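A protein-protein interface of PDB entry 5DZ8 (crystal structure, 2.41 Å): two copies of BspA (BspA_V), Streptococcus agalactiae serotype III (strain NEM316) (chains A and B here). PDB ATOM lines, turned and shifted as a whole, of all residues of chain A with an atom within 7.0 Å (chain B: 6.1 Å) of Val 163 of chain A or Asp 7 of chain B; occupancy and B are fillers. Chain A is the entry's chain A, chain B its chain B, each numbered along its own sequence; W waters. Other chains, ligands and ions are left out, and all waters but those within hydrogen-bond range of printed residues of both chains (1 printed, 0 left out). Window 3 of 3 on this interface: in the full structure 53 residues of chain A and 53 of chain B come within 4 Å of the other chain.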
ATOM      1  N   ALA A 161     -24.510  27.607 -13.199  1.00  0.00           N
ATOM      2  CA  ALA A 161     -24.408  28.222 -14.496  1.00  0.00           C
ATOM      3  C   ALA A 161     -22.988  27.984 -14.945  1.00  0.00           C
ATOM      4  O   ALA A 161     -22.045  28.396 -14.232  1.00  0.00           O
ATOM      5  CB  ALA A 161     -24.691  29.718 -14.365  1.00  0.00           C
ATOM      6  N   LEU A 162     -22.829  27.371 -16.126  1.00  0.00           N
ATOM      7  CA  LEU A 162     -21.522  26.965 -16.616  1.00  0.00           C
ATOM      8  C   LEU A 162     -21.317  27.584 -17.948  1.00  0.00           C
ATOM      9  O   LEU A 162     -22.130  27.367 -18.846  1.00  0.00           O
ATOM     10  CB  LEU A 162     -21.431  25.435 -16.736  1.00  0.00           C
ATOM     11  CG  LEU A 162     -21.604  24.657 -15.433  1.00  0.00           C
ATOM     12  CD1 LEU A 162     -22.017  23.243 -15.717  1.00  0.00           C
ATOM     13  CD2 LEU A 162     -20.337  24.632 -14.618  1.00  0.00           C
ATOM     14  N   VAL A 163     -20.228  28.328 -18.093  1.00  0.00           N
ATOM     15  CA  VAL A 163     -19.873  28.892 -19.380  1.00  0.00           C
ATOM     16  C   VAL A 163     -18.833  27.995 -20.022  1.00  0.00           C
ATOM     17  O   VAL A 163     -18.120  27.305 -19.320  1.00  0.00           O
ATOM     18  CB  VAL A 163     -19.321  30.369 -19.262  1.00  0.00           C
ATOM     19  CG1 VAL A 163     -20.361  31.262 -18.635  1.00  0.00           C
ATOM     20  CG2 VAL A 163     -17.985  30.494 -18.491  1.00  0.00           C
ATOM     21  N   SER A 164     -18.735  28.031 -21.349  1.00  0.00           N
ATOM     22  CA  SER A 164     -17.638  27.384 -22.055  1.00  0.00           C
ATOM     23  C   SER A 164     -17.215  28.134 -23.296  1.00  0.00           C
ATOM     24  O   SER A 164     -18.004  28.861 -23.918  1.00  0.00           O
ATOM     25  CB  SER A 164     -18.007  25.962 -22.422  1.00  0.00           C
ATOM     26  OG  SER A 164     -19.011  25.993 -23.417  1.00  0.00           O
ATOM     27  N   TYR A 165     -15.942  27.979 -23.621  1.00  0.00           N
ATOM     28  CA  TYR A 165     -15.325  28.627 -24.749  1.00  0.00           C
ATOM     29  C   TYR A 165     -14.454  27.628 -25.481  1.00  0.00           C
ATOM     30  O   TYR A 165     -13.622  26.969 -24.867  1.00  0.00           O
ATOM     31  CB  TYR A 165     -14.473  29.800 -24.311  1.00  0.00           C
ATOM     32  CG  TYR A 165     -15.228  30.870 -23.555  1.00  0.00           C
ATOM     33  CD1 TYR A 165     -15.429  30.757 -22.170  1.00  0.00           C
ATOM     34  CD2 TYR A 165     -15.708  32.001 -24.200  1.00  0.00           C
ATOM     35  CE1 TYR A 165     -16.179  31.697 -21.472  1.00  0.00           C
ATOM     36  CE2 TYR A 165     -16.430  32.972 -23.495  1.00  0.00           C
ATOM     37  CZ  TYR A 165     -16.646  32.827 -22.130  1.00  0.00           C
ATOM     38  OH  TYR A 165     -17.347  33.774 -21.437  1.00  0.00           O
ATOM     39  N   VAL A 166     -14.661  27.548 -26.796  1.00  0.00           N
ATOM     40  CA  VAL A 166     -13.934  26.658 -27.704  1.00  0.00           C
ATOM     41  C   VAL A 166     -13.280  27.505 -28.828  1.00  0.00           C
ATOM     42  O   VAL A 166     -13.961  28.317 -29.470  1.00  0.00           O
ATOM     43  CB  VAL A 166     -14.907  25.631 -28.327  1.00  0.00           C
ATOM     44  CG1 VAL A 166     -14.118  24.625 -29.196  1.00  0.00           C
ATOM     45  CG2 VAL A 166     -15.673  24.931 -27.212  1.00  0.00           C
ATOM     46  N   ALA B   5     -16.345  30.029 -29.967  1.00  0.00           N
ATOM     47  CA  ALA B   5     -17.737  29.756 -29.651  1.00  0.00           C
ATOM     48  C   ALA B   5     -17.967  29.791 -28.118  1.00  0.00           C
ATOM     49  O   ALA B   5     -17.327  29.070 -27.343  1.00  0.00           O
ATOM     50  CB  ALA B   5     -18.153  28.403 -30.228  1.00  0.00           C
ATOM     51  N   PHE B   6     -18.894  30.647 -27.721  1.00  0.00           N
ATOM     52  CA  PHE B   6     -19.242  30.904 -26.315  1.00  0.00           C
ATOM     53  C   PHE B   6     -20.497  30.152 -26.030  1.00  0.00           C
ATOM     54  O   PHE B   6     -21.416  30.188 -26.811  1.00  0.00           O
ATOM     55  CB  PHE B   6     -19.486  32.387 -26.074  1.00  0.00           C
ATOM     56  CG  PHE B   6     -20.368  32.675 -24.901  1.00  0.00           C
ATOM     57  CD1 PHE B   6     -19.916  32.447 -23.594  1.00  0.00           C
ATOM     58  CD2 PHE B   6     -21.644  33.189 -25.083  1.00  0.00           C
ATOM     59  CE1 PHE B   6     -20.730  32.707 -22.520  1.00  0.00           C
ATOM     60  CE2 PHE B   6     -22.475  33.442 -24.006  1.00  0.00           C
ATOM     61  CZ  PHE B   6     -22.022  33.222 -22.723  1.00  0.00           C
ATOM     62  N   ASP B   7     -20.539  29.432 -24.926  1.00  0.00           N
ATOM     63  CA  ASP B   7     -21.808  28.863 -24.474  1.00  0.00           C
ATOM     64  C   ASP B   7     -22.009  29.016 -22.981  1.00  0.00           C
ATOM     65  O   ASP B   7     -21.044  29.213 -22.229  1.00  0.00           O
ATOM     66  CB  ASP B   7     -21.934  27.408 -24.889  1.00  0.00           C
ATOM     67  CG  ASP B   7     -23.417  26.975 -25.037  1.00  0.00           C
ATOM     68  OD1 ASP B   7     -24.349  27.808 -25.391  1.00  0.00           O
ATOM     69  OD2 ASP B   7     -23.651  25.775 -24.767  1.00  0.00           O
ATOM     70  N   ILE B   8     -23.267  29.000 -22.564  1.00  0.00           N
ATOM     71  CA  ILE B   8     -23.599  28.982 -21.146  1.00  0.00           C
ATOM     72  C   ILE B   8     -24.817  28.095 -20.914  1.00  0.00           C
ATOM     73  O   ILE B   8     -25.833  28.257 -21.589  1.00  0.00           O
ATOM     74  CB  ILE B   8     -23.819  30.402 -20.532  1.00  0.00           C
ATOM     75  CG1 ILE B   8     -23.962  30.293 -19.000  1.00  0.00           C
ATOM     76  CG2 ILE B   8     -25.065  31.075 -21.091  1.00  0.00           C
ATOM     77  CD1 ILE B   8     -23.993  31.615 -18.270  1.00  0.00           C
ATOM     78  N   LYS B   9     -24.710  27.218 -19.921  1.00  0.00           N
ATOM     79  CA  LYS B   9     -25.694  26.133 -19.635  1.00  0.00           C
ATOM     80  C   LYS B   9     -25.958  26.022 -18.106  1.00  0.00           C
ATOM     81  O   LYS B   9     -25.180  26.531 -17.296  1.00  0.00           O
ATOM     82  CB  LYS B   9     -25.176  24.769 -20.144  1.00  0.00           C
ATOM     83  N   THR B  29     -29.092  32.742 -25.638  1.00  0.00           N
ATOM     84  CA  THR B  29     -27.703  33.181 -25.579  1.00  0.00           C
ATOM     85  C   THR B  29     -27.291  33.946 -26.855  1.00  0.00           C
ATOM     86  O   THR B  29     -27.715  33.620 -27.964  1.00  0.00           O
ATOM     87  CB  THR B  29     -26.703  32.010 -25.427  1.00  0.00           C
ATOM     88  OG1 THR B  29     -26.659  31.242 -26.630  1.00  0.00           O
ATOM     89  CG2 THR B  29     -27.078  31.084 -24.306  1.00  0.00           C
ATOM     90  N   VAL B  57     -22.635  37.650 -19.469  1.00  0.00           N
ATOM     91  CA  VAL B  57     -21.248  37.380 -19.214  1.00  0.00           C
ATOM     92  C   VAL B  57     -20.400  38.447 -19.894  1.00  0.00           C
ATOM     93  O   VAL B  57     -20.625  38.737 -21.069  1.00  0.00           O
ATOM     94  CB  VAL B  57     -20.859  36.009 -19.721  1.00  0.00           C
ATOM     95  CG1 VAL B  57     -19.377  35.763 -19.446  1.00  0.00           C
ATOM     96  CG2 VAL B  57     -21.727  34.955 -19.025  1.00  0.00           C
ATOM     97  N   VAL B  73     -12.555  36.096 -19.324  1.00  0.00           N
ATOM     98  CA  VAL B  73     -13.882  36.055 -18.762  1.00  0.00           C
ATOM     99  C   VAL B  73     -13.871  36.947 -17.528  1.00  0.00           C
ATOM    100  O   VAL B  73     -13.503  36.517 -16.414  1.00  0.00           O
ATOM    101  CB  VAL B  73     -14.361  34.638 -18.457  1.00  0.00           C
ATOM    102  CG1 VAL B  73     -15.890  34.626 -18.308  1.00  0.00           C
ATOM    103  CG2 VAL B  73     -13.995  33.709 -19.578  1.00  0.00           C
ATOM    104  N   TYR B 133      -8.614  32.135 -20.214  1.00  0.00           N
ATOM    105  CA  TYR B 133      -8.274  30.841 -20.914  1.00  0.00           C
ATOM    106  C   TYR B 133      -7.438  31.051 -22.152  1.00  0.00           C
ATOM    107  O   TYR B 133      -7.898  31.625 -23.107  1.00  0.00           O
ATOM    108  CB  TYR B 133      -9.559  30.072 -21.261  1.00  0.00           C
ATOM    109  CG  TYR B 133     -10.297  29.879 -19.978  1.00  0.00           C
ATOM    110  CD1 TYR B 133      -9.911  28.905 -19.094  1.00  0.00           C
ATOM    111  CD2 TYR B 133     -11.319  30.778 -19.593  1.00  0.00           C
ATOM    112  CE1 TYR B 133     -10.550  28.777 -17.859  1.00  0.00           C
ATOM    113  CE2 TYR B 133     -11.971  30.656 -18.382  1.00  0.00           C
ATOM    114  CZ  TYR B 133     -11.580  29.657 -17.518  1.00  0.00           C
ATOM    115  OH  TYR B 133     -12.203  29.535 -16.309  1.00  0.00           O
ATOM    116  N   SER B 141     -12.059  25.702 -22.835  1.00  0.00           N
ATOM    117  CA  SER B 141     -12.018  26.080 -21.433  1.00  0.00           C
ATOM    118  C   SER B 141     -12.590  24.990 -20.549  1.00  0.00           C
ATOM    119  O   SER B 141     -12.308  24.963 -19.386  1.00  0.00           O
ATOM    120  CB  SER B 141     -12.894  27.335 -21.194  1.00  0.00           C
ATOM    121  OG  SER B 141     -14.260  27.092 -21.603  1.00  0.00           O
ATOM    122  N   GLY B 142     -13.394  24.107 -21.105  1.00  0.00           N
ATOM    123  CA  GLY B 142     -14.243  23.253 -20.310  1.00  0.00           C
ATOM    124  C   GLY B 142     -15.353  24.062 -19.655  1.00  0.00           C
ATOM    125  O   GLY B 142     -15.584  25.261 -19.983  1.00  0.00           O
ATOM    126  N   ASN B 143     -16.027  23.400 -18.721  1.00  0.00           N
ATOM    127  CA  ASN B 143     -17.175  23.967 -18.039  1.00  0.00           C
ATOM    128  C   ASN B 143     -16.707  24.788 -16.877  1.00  0.00           C
ATOM    129  O   ASN B 143     -16.093  24.278 -15.955  1.00  0.00           O
ATOM    130  CB  ASN B 143     -18.091  22.867 -17.548  1.00  0.00           C
ATOM    131  CG  ASN B 143     -18.774  22.128 -18.670  1.00  0.00           C
ATOM    132  OD1 ASN B 143     -19.053  22.676 -19.738  1.00  0.00           O
ATOM    133  ND2 ASN B 143     -19.047  20.859 -18.434  1.00  0.00           N
ATOM    134  N   VAL B 144     -16.969  26.065 -16.937  1.00  0.00           N
ATOM    135  CA  VAL B 144     -16.527  26.975 -15.868  1.00  0.00           C
ATOM    136  C   VAL B 144     -17.723  27.510 -15.122  1.00  0.00           C
ATOM    137  O   VAL B 144     -18.603  28.104 -15.717  1.00  0.00           O
ATOM    138  CB  VAL B 144     -15.719  28.122 -16.478  1.00  0.00           C
ATOM    139  CG1 VAL B 144     -15.077  28.932 -15.394  1.00  0.00           C
ATOM    140  CG2 VAL B 144     -14.690  27.546 -17.445  1.00  0.00           C
ATOM    141  N   GLU B 145     -17.796  27.238 -13.838  1.00  0.00           N
ATOM    142  CA  GLU B 145     -18.973  27.673 -13.071  1.00  0.00           C
ATOM    143  C   GLU B 145     -18.875  29.177 -12.855  1.00  0.00           C
ATOM    144  O   GLU B 145     -17.847  29.670 -12.382  1.00  0.00           O
ATOM    145  CB  GLU B 145     -19.056  26.947 -11.743  1.00  0.00           C
ATOM    146  CG  GLU B 145     -20.238  27.348 -10.858  1.00  0.00           C
ATOM    147  CD  GLU B 145     -20.365  26.445  -9.613  1.00  0.00           C
ATOM    148  OE1 GLU B 145     -19.389  26.376  -8.827  1.00  0.00           O
ATOM    149  OE2 GLU B 145     -21.410  25.783  -9.402  1.00  0.00           O
ATOM    150  N   VAL B 146     -19.914  29.928 -13.201  1.00  0.00           N
ATOM    151  CA  VAL B 146     -19.856  31.354 -12.935  1.00  0.00           C
ATOM    152  C   VAL B 146     -20.803  31.873 -11.818  1.00  0.00           C
ATOM    153  O   VAL B 146     -20.590  32.923 -11.271  1.00  0.00           O
ATOM    154  CB  VAL B 146     -19.971  32.157 -14.233  1.00  0.00           C
ATOM    155  CG1 VAL B 146     -18.736  31.879 -15.156  1.00  0.00           C
ATOM    156  CG2 VAL B 146     -21.313  31.931 -14.951  1.00  0.00           C
HETATM  157  O   HOH W   1     -18.663  26.754 -26.252  1.00  0.00           O
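N of Tyr 165 of chain A sits at hydrogen-bond distance from OG of Ser 141 of chain B, 2.8 Å away.
N of Val 146 of chain B lies within hydrogen-bond range of O of Ala 161 of chain A.
The backbone NH (N) of Ser 164 of chain A sits at hydrogen-bond distance from the backbone carbonyl oxygen (O) of Asp 7 of chain B.
The backbone NH of Val 163 of chain A lies within hydrogen-bond range of the backbone carbonyl oxygen of Val 144 of chain B (2.9 Å).
The backbone carbonyl oxygen (O) of Ala 5 of chain B sits close to the backbone carbonyl oxygen (O) of Ser 164 of chain A, 3.5 Å away.
O of Lys 9 of chain B lies within hydrogen-bond range of N of Leu 162 of chain A.
The backbone NH (N) of Ala 5 of chain B is in hydrogen-bond range of the backbone carbonyl oxygen (O) of Val 166 of chain A (3.0 Å).
O of Gly 142 of chain B sits close to O of Val 163 of chain A, at 3.3 Å.
Among the printed residues, pairs that only touch across the chains: Val 163 of chain A with Asp 7 of chain B (3.1 Å), Leu 162 of chain A with Ile 8 of chain B (3.2 Å), Leu 162 of chain A with Val 144 of chain B (3.3 Å), Tyr 165 of chain A with Ala 5 of chain B (3.3 Å), Ala 161 of chain A with Lys 9 of chain B (3.4 Å), Ala 161 of chain A with Glu 145 of chain B (3.4 Å), Ser 164 of chain A with Phe 6 of chain B (3.4 Å), Ser 164 of chain A with Ser 141 of chain B (3.4 Å), Tyr 165 of chain A with Val 57 of chain B (3.5 Å), Ser 164 of chain A with Gly 142 of chain B (3.5 Å), Tyr 165 of chain A with Val 73 of chain B (3.5 Å), Tyr 165 of chain A with Phe 6 of chain B (3.5 Å), Val 163 of chain A with Ile 8 of chain B (3.7 Å), Leu 162 of chain A with Glu 145 of chain B (3.7 Å), Val 163 of chain A with Val 146 of chain B (3.7 Å), Val 163 of chain A with Asn 143 of chain B (3.7 Å), Ala 161 of chain A with Val 144 of chain B (3.8 Å) and Val 163 of chain A with Val 57 of chain B (3.96 Å).
Of chain B, only Asp 7 (3.1 Å), Ile 8 (3.7 Å), Val 57 (3.96 Å), Gly 142 (3.3 Å), Asn 143 (3.7 Å), Val 144 (2.9 Å) and Val 146 (3.7 Å) come within 4 Å of Val 163 of chain A.
Of the printed residues of chain A, Asp 7 of chain B touches Val 163 and Ser 164.
Of the printed residues of chain A, Val 57 of chain B touches Val 163 (3.96 Å) and Tyr 165 (3.5 Å).
Of the printed residues of chain B, Ser 164 of chain A touches Ala 5, Phe 6, Asp 7, Ser 141 and Gly 142.
Printed residues of chain A within 4 Å of Asn 143 of chain B: Val 163 (3.7 Å).
Of the printed residues of chain A, Val 73 of chain B touches Tyr 165.
Of the printed residues of chain A, Ala 5 of chain B touches Ser 164, Tyr 165 and Val 166.
Tyr 133 of chain B touches none of the printed residues of chain A.
The nearest residue of chain B that does not touch Val 163 of chain A is Phe 6 of chain B (4.2 Å).
Hydrophobic or aromatic side chains of chain B that line the printed part of chain A: Phe 6, Ile 8, Val 57, Val 73, Val 144 and Val 146.
Of the 6 printed residues of chain A, 6 touch a printed residue of chain B.
Among the printed residues, 26 pairs touch across the chains.
No position is printed for both chains.
Water W1 lies within hydrogen-bond range of the backbone carbonyl oxygen (O) of Ala 5 of chain B (2.9 Å) and the side-chain hydroxyl (OG) of Ser 164 of chain A (3.0 Å).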
